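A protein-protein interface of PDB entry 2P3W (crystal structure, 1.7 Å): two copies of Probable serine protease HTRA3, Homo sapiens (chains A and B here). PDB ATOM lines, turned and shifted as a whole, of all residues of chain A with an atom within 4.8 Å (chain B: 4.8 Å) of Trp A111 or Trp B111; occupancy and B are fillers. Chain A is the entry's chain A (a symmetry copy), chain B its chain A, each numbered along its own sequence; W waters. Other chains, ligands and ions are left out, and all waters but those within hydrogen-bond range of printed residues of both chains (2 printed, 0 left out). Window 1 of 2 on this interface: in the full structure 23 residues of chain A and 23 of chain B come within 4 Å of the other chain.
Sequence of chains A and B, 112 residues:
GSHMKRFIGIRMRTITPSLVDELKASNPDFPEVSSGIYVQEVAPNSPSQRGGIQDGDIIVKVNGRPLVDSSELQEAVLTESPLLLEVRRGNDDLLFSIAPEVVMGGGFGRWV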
ATOM      1  N   GLY A   9     -15.572 -25.913  12.620  1.00  0.00           N
ATOM      2  CA  GLY A   9     -15.312 -24.803  11.727  1.00  0.00           C
ATOM      3  C   GLY A   9     -14.390 -25.071  10.550  1.00  0.00           C
ATOM      4  O   GLY A   9     -13.542 -24.233  10.210  1.00  0.00           O
ATOM      5  N   ILE A  10     -14.566 -26.220   9.905  1.00  0.00           N
ATOM      6  CA  ILE A  10     -13.896 -26.449   8.629  1.00  0.00           C
ATOM      7  C   ILE A  10     -14.891 -26.903   7.588  1.00  0.00           C
ATOM      8  O   ILE A  10     -15.897 -27.546   7.937  1.00  0.00           O
ATOM      9  CB  ILE A  10     -12.745 -27.467   8.747  1.00  0.00           C
ATOM     10  CG1 ILE A  10     -13.245 -28.836   9.157  1.00  0.00           C
ATOM     11  CG2 ILE A  10     -11.672 -27.023   9.738  1.00  0.00           C
ATOM     12  CD1 ILE A  10     -12.167 -29.932   8.963  1.00  0.00           C
ATOM     13  N   ARG A  11     -14.597 -26.587   6.318  1.00  0.00           N
ATOM     14  CA  ARG A  11     -15.318 -27.178   5.194  1.00  0.00           C
ATOM     15  C   ARG A  11     -14.404 -28.298   4.667  1.00  0.00           C
ATOM     16  O   ARG A  11     -13.272 -28.055   4.272  1.00  0.00           O
ATOM     17  CB  ARG A  11     -15.672 -26.132   4.141  1.00  0.00           C
ATOM     18  CG  ARG A  11     -16.425 -26.760   2.964  1.00  0.00           C
ATOM     19  CD  ARG A  11     -17.475 -25.866   2.371  1.00  0.00           C
ATOM     20  NE  ARG A  11     -16.934 -24.636   1.802  1.00  0.00           N
ATOM     21  CZ  ARG A  11     -16.317 -24.559   0.639  1.00  0.00           C
ATOM     22  NH1 ARG A  11     -16.141 -25.641  -0.087  1.00  0.00           N
ATOM     23  NH2 ARG A  11     -15.890 -23.379   0.190  1.00  0.00           N
ATOM     24  N   GLU A  41     -11.659 -25.192   3.593  1.00  0.00           N
ATOM     25  CA  GLU A  41     -11.744 -23.856   4.201  1.00  0.00           C
ATOM     26  C   GLU A  41     -11.788 -23.961   5.739  1.00  0.00           C
ATOM     27  O   GLU A  41     -12.228 -24.973   6.293  1.00  0.00           O
ATOM     28  CB  GLU A  41     -13.004 -23.105   3.731  1.00  0.00           C
ATOM     29  CG  GLU A  41     -13.169 -22.888   2.244  1.00  0.00           C
ATOM     30  CD  GLU A  41     -12.091 -22.007   1.613  1.00  0.00           C
ATOM     31  OE1 GLU A  41     -11.890 -22.160   0.376  1.00  0.00           O
ATOM     32  OE2 GLU A  41     -11.457 -21.180   2.332  1.00  0.00           O
ATOM     33  N   VAL A  42     -11.287 -22.912   6.404  1.00  0.00           N
ATOM     34  CA  VAL A  42     -11.419 -22.773   7.860  1.00  0.00           C
ATOM     35  C   VAL A  42     -12.245 -21.538   8.183  1.00  0.00           C
ATOM     36  O   VAL A  42     -11.971 -20.434   7.673  1.00  0.00           O
ATOM     37  CB  VAL A  42     -10.030 -22.646   8.536  1.00  0.00           C
ATOM     38  CG1 VAL A  42     -10.185 -22.572  10.043  1.00  0.00           C
ATOM     39  CG2 VAL A  42      -9.118 -23.803   8.122  1.00  0.00           C
ATOM     40  N   ALA A  43     -13.286 -21.701   8.997  1.00  0.00           N
ATOM     41  CA  ALA A  43     -14.110 -20.560   9.392  1.00  0.00           C
ATOM     42  C   ALA A  43     -13.360 -19.668  10.415  1.00  0.00           C
ATOM     43  O   ALA A  43     -12.640 -20.178  11.274  1.00  0.00           O
ATOM     44  CB  ALA A  43     -15.466 -21.021   9.949  1.00  0.00           C
ATOM     45  N   PHE A 108     -26.869 -21.290  16.212  1.00  0.00           N
ATOM     46  CA  PHE A 108     -25.855 -21.535  15.158  1.00  0.00           C
ATOM     47  C   PHE A 108     -26.278 -20.978  13.808  1.00  0.00           C
ATOM     48  O   PHE A 108     -25.467 -20.480  13.015  1.00  0.00           O
ATOM     49  CB  PHE A 108     -25.627 -23.026  15.021  1.00  0.00           C
ATOM     50  CG  PHE A 108     -24.505 -23.401  14.087  1.00  0.00           C
ATOM     51  CD1 PHE A 108     -23.182 -23.169  14.422  1.00  0.00           C
ATOM     52  CD2 PHE A 108     -24.788 -24.001  12.854  1.00  0.00           C
ATOM     53  CE1 PHE A 108     -22.163 -23.541  13.561  1.00  0.00           C
ATOM     54  CE2 PHE A 108     -23.771 -24.375  11.985  1.00  0.00           C
ATOM     55  CZ  PHE A 108     -22.455 -24.146  12.341  1.00  0.00           C
ATOM     56  N   GLY A 109     -27.559 -21.092  13.511  1.00  0.00           N
ATOM     57  CA  GLY A 109     -28.033 -20.715  12.170  1.00  0.00           C
ATOM     58  C   GLY A 109     -27.625 -21.761  11.149  1.00  0.00           C
ATOM     59  O   GLY A 109     -27.624 -22.959  11.444  1.00  0.00           O
ATOM     60  N   ARG A 110     -27.292 -21.314   9.942  1.00  0.00           N
ATOM     61  CA  ARG A 110     -26.739 -22.216   8.946  1.00  0.00           C
ATOM     62  C   ARG A 110     -25.916 -21.528   7.898  1.00  0.00           C
ATOM     63  O   ARG A 110     -26.168 -20.376   7.572  1.00  0.00           O
ATOM     64  CB  ARG A 110     -27.815 -23.041   8.261  1.00  0.00           C
ATOM     65  CG  ARG A 110     -28.778 -22.311   7.432  1.00  0.00           C
ATOM     66  CD  ARG A 110     -29.720 -23.347   6.780  1.00  0.00           C
ATOM     67  NE  ARG A 110     -30.796 -22.720   6.037  1.00  0.00           N
ATOM     68  CZ  ARG A 110     -31.888 -22.188   6.582  1.00  0.00           C
ATOM     69  NH1 ARG A 110     -32.063 -22.167   7.898  1.00  0.00           N
ATOM     70  NH2 ARG A 110     -32.811 -21.652   5.800  1.00  0.00           N
ATOM     71  N   TRP A 111     -24.966 -22.291   7.351  1.00  0.00           N
ATOM     72  CA  TRP A 111     -24.110 -21.832   6.263  1.00  0.00           C
ATOM     73  C   TRP A 111     -24.910 -21.777   4.983  1.00  0.00           C
ATOM     74  O   TRP A 111     -25.788 -22.632   4.741  1.00  0.00           O
ATOM     75  CB  TRP A 111     -22.905 -22.763   6.079  1.00  0.00           C
ATOM     76  CG  TRP A 111     -21.868 -22.556   7.091  1.00  0.00           C
ATOM     77  CD1 TRP A 111     -21.587 -23.337   8.172  1.00  0.00           C
ATOM     78  CD2 TRP A 111     -20.941 -21.475   7.120  1.00  0.00           C
ATOM     79  NE1 TRP A 111     -20.538 -22.796   8.878  1.00  0.00           N
ATOM     80  CE2 TRP A 111     -20.118 -21.659   8.244  1.00  0.00           C
ATOM     81  CE3 TRP A 111     -20.710 -20.389   6.287  1.00  0.00           C
ATOM     82  CZ2 TRP A 111     -19.101 -20.781   8.564  1.00  0.00           C
ATOM     83  CZ3 TRP A 111     -19.705 -19.508   6.607  1.00  0.00           C
ATOM     84  CH2 TRP A 111     -18.918 -19.709   7.745  1.00  0.00           C
ATOM     85  N   VAL A 112     -24.607 -20.768   4.180  1.00  0.00           N
ATOM     86  CA  VAL A 112     -25.210 -20.618   2.855  1.00  0.00           C
ATOM     87  C   VAL A 112     -24.228 -19.973   1.887  1.00  0.00           C
ATOM     88  O   VAL A 112     -24.479 -19.918   0.662  1.00  0.00           O
ATOM     89  CB  VAL A 112     -26.506 -19.756   2.960  1.00  0.00           C
ATOM     90  CG1 VAL A 112     -26.195 -18.293   3.211  1.00  0.00           C
ATOM     91  CG2 VAL A 112     -27.386 -19.934   1.755  1.00  0.00           C
ATOM     92  OXT VAL A 112     -23.175 -19.493   2.346  1.00  0.00           O
ATOM     93  N   GLY B   9     -21.246 -17.883   1.184  1.00  0.00           N
ATOM     94  CA  GLY B   9     -20.244 -17.884   2.230  1.00  0.00           C
ATOM     95  C   GLY B   9     -20.560 -17.081   3.481  1.00  0.00           C
ATOM     96  O   GLY B   9     -19.681 -16.400   4.031  1.00  0.00           O
ATOM     97  N   ILE B  10     -21.799 -17.177   3.955  1.00  0.00           N
ATOM     98  CA  ILE B  10     -22.118 -16.640   5.273  1.00  0.00           C
ATOM     99  C   ILE B  10     -22.824 -17.682   6.107  1.00  0.00           C
ATOM    100  O   ILE B  10     -23.527 -18.544   5.550  1.00  0.00           O
ATOM    101  CB  ILE B  10     -22.967 -15.357   5.191  1.00  0.00           C
ATOM    102  CG1 ILE B  10     -24.317 -15.615   4.556  1.00  0.00           C
ATOM    103  CG2 ILE B  10     -22.270 -14.242   4.416  1.00  0.00           C
ATOM    104  CD1 ILE B  10     -25.294 -14.430   4.763  1.00  0.00           C
ATOM    105  N   ARG B  11     -22.651 -17.587   7.434  1.00  0.00           N
ATOM    106  CA  ARG B  11     -23.470 -18.352   8.371  1.00  0.00           C
ATOM    107  C   ARG B  11     -24.536 -17.365   8.879  1.00  0.00           C
ATOM    108  O   ARG B  11     -24.216 -16.331   9.450  1.00  0.00           O
ATOM    109  CB  ARG B  11     -22.627 -18.966   9.484  1.00  0.00           C
ATOM    110  CG  ARG B  11     -23.493 -19.764  10.463  1.00  0.00           C
ATOM    111  CD  ARG B  11     -22.818 -20.988  11.011  1.00  0.00           C
ATOM    112  NE  ARG B  11     -21.621 -20.689  11.791  1.00  0.00           N
ATOM    113  CZ  ARG B  11     -21.632 -20.231  13.027  1.00  0.00           C
ATOM    114  NH1 ARG B  11     -22.774 -20.000  13.636  1.00  0.00           N
ATOM    115  NH2 ARG B  11     -20.481 -20.024  13.669  1.00  0.00           N
ATOM    116  N   GLU B  41     -21.302 -15.211  10.681  1.00  0.00           N
ATOM    117  CA  GLU B  41     -19.915 -15.402  10.230  1.00  0.00           C
ATOM    118  C   GLU B  41     -19.816 -15.247   8.700  1.00  0.00           C
ATOM    119  O   GLU B  41     -20.787 -15.478   7.973  1.00  0.00           O
ATOM    120  CB  GLU B  41     -19.390 -16.799  10.611  1.00  0.00           C
ATOM    121  CG  GLU B  41     -19.398 -17.168  12.077  1.00  0.00           C
ATOM    122  CD  GLU B  41     -18.490 -16.302  12.950  1.00  0.00           C
ATOM    123  OE1 GLU B  41     -18.785 -16.232  14.176  1.00  0.00           O
ATOM    124  OE2 GLU B  41     -17.504 -15.703  12.428  1.00  0.00           O
ATOM    125  N   VAL B  42     -18.634 -14.816   8.239  1.00  0.00           N
ATOM    126  CA  VAL B  42     -18.315 -14.790   6.806  1.00  0.00           C
ATOM    127  C   VAL B  42     -17.153 -15.730   6.524  1.00  0.00           C
ATOM    128  O   VAL B  42     -16.104 -15.670   7.195  1.00  0.00           O
ATOM    129  CB  VAL B  42     -17.933 -13.360   6.346  1.00  0.00           C
ATOM    130  CG1 VAL B  42     -17.674 -13.342   4.851  1.00  0.00           C
ATOM    131  CG2 VAL B  42     -19.021 -12.357   6.738  1.00  0.00           C
ATOM    132  N   ALA B  43     -17.325 -16.635   5.562  1.00  0.00           N
ATOM    133  CA  ALA B  43     -16.246 -17.551   5.198  1.00  0.00           C
ATOM    134  C   ALA B  43     -15.142 -16.811   4.401  1.00  0.00           C
ATOM    135  O   ALA B  43     -15.442 -15.932   3.592  1.00  0.00           O
ATOM    136  CB  ALA B  43     -16.784 -18.756   4.410  1.00  0.00           C
ATOM    137  N   PHE B 108     -17.543 -29.188  -3.331  1.00  0.00           N
ATOM    138  CA  PHE B 108     -17.808 -28.283  -2.187  1.00  0.00           C
ATOM    139  C   PHE B 108     -17.494 -28.936  -0.850  1.00  0.00           C
ATOM    140  O   PHE B 108     -17.016 -28.300   0.100  1.00  0.00           O
ATOM    141  CB  PHE B 108     -19.266 -27.875  -2.200  1.00  0.00           C
ATOM    142  CG  PHE B 108     -19.630 -26.833  -1.173  1.00  0.00           C
ATOM    143  CD1 PHE B 108     -19.199 -25.522  -1.295  1.00  0.00           C
ATOM    144  CD2 PHE B 108     -20.421 -27.178  -0.071  1.00  0.00           C
ATOM    145  CE1 PHE B 108     -19.562 -24.573  -0.354  1.00  0.00           C
ATOM    146  CE2 PHE B 108     -20.786 -26.231   0.878  1.00  0.00           C
ATOM    147  CZ  PHE B 108     -20.357 -24.925   0.734  1.00  0.00           C
ATOM    148  N   GLY B 109     -17.797 -30.217  -0.745  1.00  0.00           N
ATOM    149  CA  GLY B 109     -17.665 -30.894   0.554  1.00  0.00           C
ATOM    150  C   GLY B 109     -18.784 -30.474   1.489  1.00  0.00           C
ATOM    151  O   GLY B 109     -19.922 -30.276   1.055  1.00  0.00           O
ATOM    152  N   ARG B 110     -18.469 -30.351   2.774  1.00  0.00           N
ATOM    153  CA  ARG B 110     -19.427 -29.805   3.721  1.00  0.00           C
ATOM    154  C   ARG B 110     -18.796 -29.213   4.946  1.00  0.00           C
ATOM    155  O   ARG B 110     -17.737 -29.655   5.371  1.00  0.00           O
ATOM    156  CB  ARG B 110     -20.459 -30.834   4.150  1.00  0.00           C
ATOM    157  CG  ARG B 110     -19.967 -31.979   4.922  1.00  0.00           C
ATOM    158  CD  ARG B 110     -21.186 -32.843   5.311  1.00  0.00           C
ATOM    159  NE  ARG B 110     -20.796 -34.076   5.970  1.00  0.00           N
ATOM    160  CZ  ARG B 110     -20.328 -35.156   5.349  1.00  0.00           C
ATOM    161  NH1 ARG B 110     -20.149 -35.174   4.034  1.00  0.00           N
ATOM    162  NH2 ARG B 110     -20.016 -36.230   6.056  1.00  0.00           N
ATOM    163  N   TRP B 111     -19.508 -28.241   5.522  1.00  0.00           N
ATOM    164  CA  TRP B 111     -19.104 -27.591   6.763  1.00  0.00           C
ATOM    165  C   TRP B 111     -19.318 -28.539   7.920  1.00  0.00           C
ATOM    166  O   TRP B 111     -20.296 -29.316   7.936  1.00  0.00           O
ATOM    167  CB  TRP B 111     -19.903 -26.303   6.996  1.00  0.00           C
ATOM    168  CG  TRP B 111     -19.438 -25.190   6.168  1.00  0.00           C
ATOM    169  CD1 TRP B 111     -20.026 -24.678   5.049  1.00  0.00           C
ATOM    170  CD2 TRP B 111     -18.262 -24.419   6.394  1.00  0.00           C
ATOM    171  NE1 TRP B 111     -19.275 -23.635   4.562  1.00  0.00           N
ATOM    172  CE2 TRP B 111     -18.193 -23.451   5.378  1.00  0.00           C
ATOM    173  CE3 TRP B 111     -17.280 -24.438   7.375  1.00  0.00           C
ATOM    174  CZ2 TRP B 111     -17.166 -22.530   5.308  1.00  0.00           C
ATOM    175  CZ3 TRP B 111     -16.251 -23.530   7.302  1.00  0.00           C
ATOM    176  CH2 TRP B 111     -16.201 -22.592   6.265  1.00  0.00           C
ATOM    177  N   VAL B 112     -18.399 -28.472   8.871  1.00  0.00           N
ATOM    178  CA  VAL B 112     -18.502 -29.244  10.111  1.00  0.00           C
ATOM    179  C   VAL B 112     -17.884 -28.481  11.273  1.00  0.00           C
ATOM    180  O   VAL B 112     -18.026 -28.882  12.450  1.00  0.00           O
ATOM    181  CB  VAL B 112     -17.794 -30.623   9.934  1.00  0.00           C
ATOM    182  CG1 VAL B 112     -16.283 -30.483   9.905  1.00  0.00           C
ATOM    183  CG2 VAL B 112     -18.236 -31.608  10.978  1.00  0.00           C
ATOM    184  OXT VAL B 112     -17.225 -27.455  11.022  1.00  0.00           O
HETATM  185  O   HOH W   1     -19.161 -25.292  10.777  1.00  0.00           O
HETATM  186  O   HOH W   2     -21.309 -21.717   2.583  1.00  0.00           O
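N of Gly B9 is in hydrogen-bond range of OXT of Val A112 (2.8 Å).
The backbone carbonyl oxygen of Ile B10 is in hydrogen-bond range of the backbone NH of Val A112 (2.8 Å).
The backbone carbonyl oxygen of Phe A108 lies within hydrogen-bond range of the guanidinium group of Arg B11, at 2.8 Å.
NH1 of Arg A11 lies within hydrogen-bond range of O of Phe B108, at 2.8 Å.
The backbone NH (N) of Gly A9 sits at hydrogen-bond distance from the chain-end carboxylate (OXT) of Val B112, at 2.8 Å.
The backbone NH (N) of Val B112 is in hydrogen-bond range of the backbone carbonyl oxygen (O) of Ile A10 (2.8 Å).
O of Ile A10 touches O of Arg B110, at 3.8 Å.
Trp B111 touches Ile A10 (CA to O, 3.4 Å).
Arg A11 touches Arg B110 (CA to O, 3.5 Å).
N of Arg A11 touches CE3 of Trp B111 (3.6 Å).
CZ3 of Trp B111 touches CB of Ala A43 (3.7 Å).
Ile B10 touches Arg A110.
Arg A110 touches Arg B11.
O of Ile B10 touches CA of Trp A111, 3.4 Å away.
Ala B43 touches Trp A111.
CG of Trp A111 touches CD1 of Trp B111, 3.5 Å away.
Water W1 lies within hydrogen-bond range of OXT of Val B112 (2.9 Å) and NE1 of Trp A111 (3.4 Å).
Water W2 lies within hydrogen-bond range of OXT of Val A112 (2.9 Å) and NE1 of Trp B111 (3.4 Å).
Of chain B, only Ile B10, Arg B11, Ala B43 and Trp B111 come within 4 Å of Trp A111.
Printed residues of chain B within 4 Å of Ile A10: Arg B110 (3.8 Å), Trp B111 (3.4 Å) and Val B112 (2.8 Å).
Of the printed residues of chain B, Arg A11 touches Phe B108, Arg B110 and Trp B111.
Printed residues of chain A within 4 Å of Val B112: Gly A9 and Ile A10.
Glu B41 touches none of the printed residues of chain A.
Val A42 touches none of the printed residues of chain B.
The nearest residue of chain B that does not touch Trp A111 is Gly B9 (4.04 Å).
The nearest residue of chain A that does not touch Trp B111 is Gly A9 (4.04 Å).
Ile A10 touches Arg B110, and with the chains exchanged Arg A110 touches Ile B10.
Arg A11 touches Phe B108, and with the chains exchanged Phe A108 touches Arg B11.
Ala A43 touches Trp B111, and with the chains exchanged Trp A111 touches Ala B43.
Trp B111 touches its own counterpart, Trp A111.
11 positions are printed for both chains.
Of the 17 pairs that touch across the chains among the printed residues, 17 have their exchanged pair printed and touching as well.
Hydrophobic or aromatic side chains of chain A that line the printed part of chain B: Ile A10, Ala A43, Phe A108, Trp A111 and Val A112.
Hydrophobic or aromatic side chains of chain B that line the printed part of chain A: Ile B10, Ala B43, Phe B108, Trp B111 and Val B112.
Among the printed residues, 17 pairs touch across the chains.
Among the printed residues, no Asp or Glu carboxylate lies within 4 Å of a Lys or Arg side-chain nitrogen of the other chain.
N of Ala B43 is in hydrogen-bond range of O of Gly B9 (2.8 Å).
N of Arg B11 is in hydrogen-bond range of O of Glu B41 (2.9 Å).
O of Gly A9 is in hydrogen-bond range of N of Ala A43, 2.8 Å away.
N of Arg A11 sits at hydrogen-bond distance from O of Glu A41 (2.9 Å).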
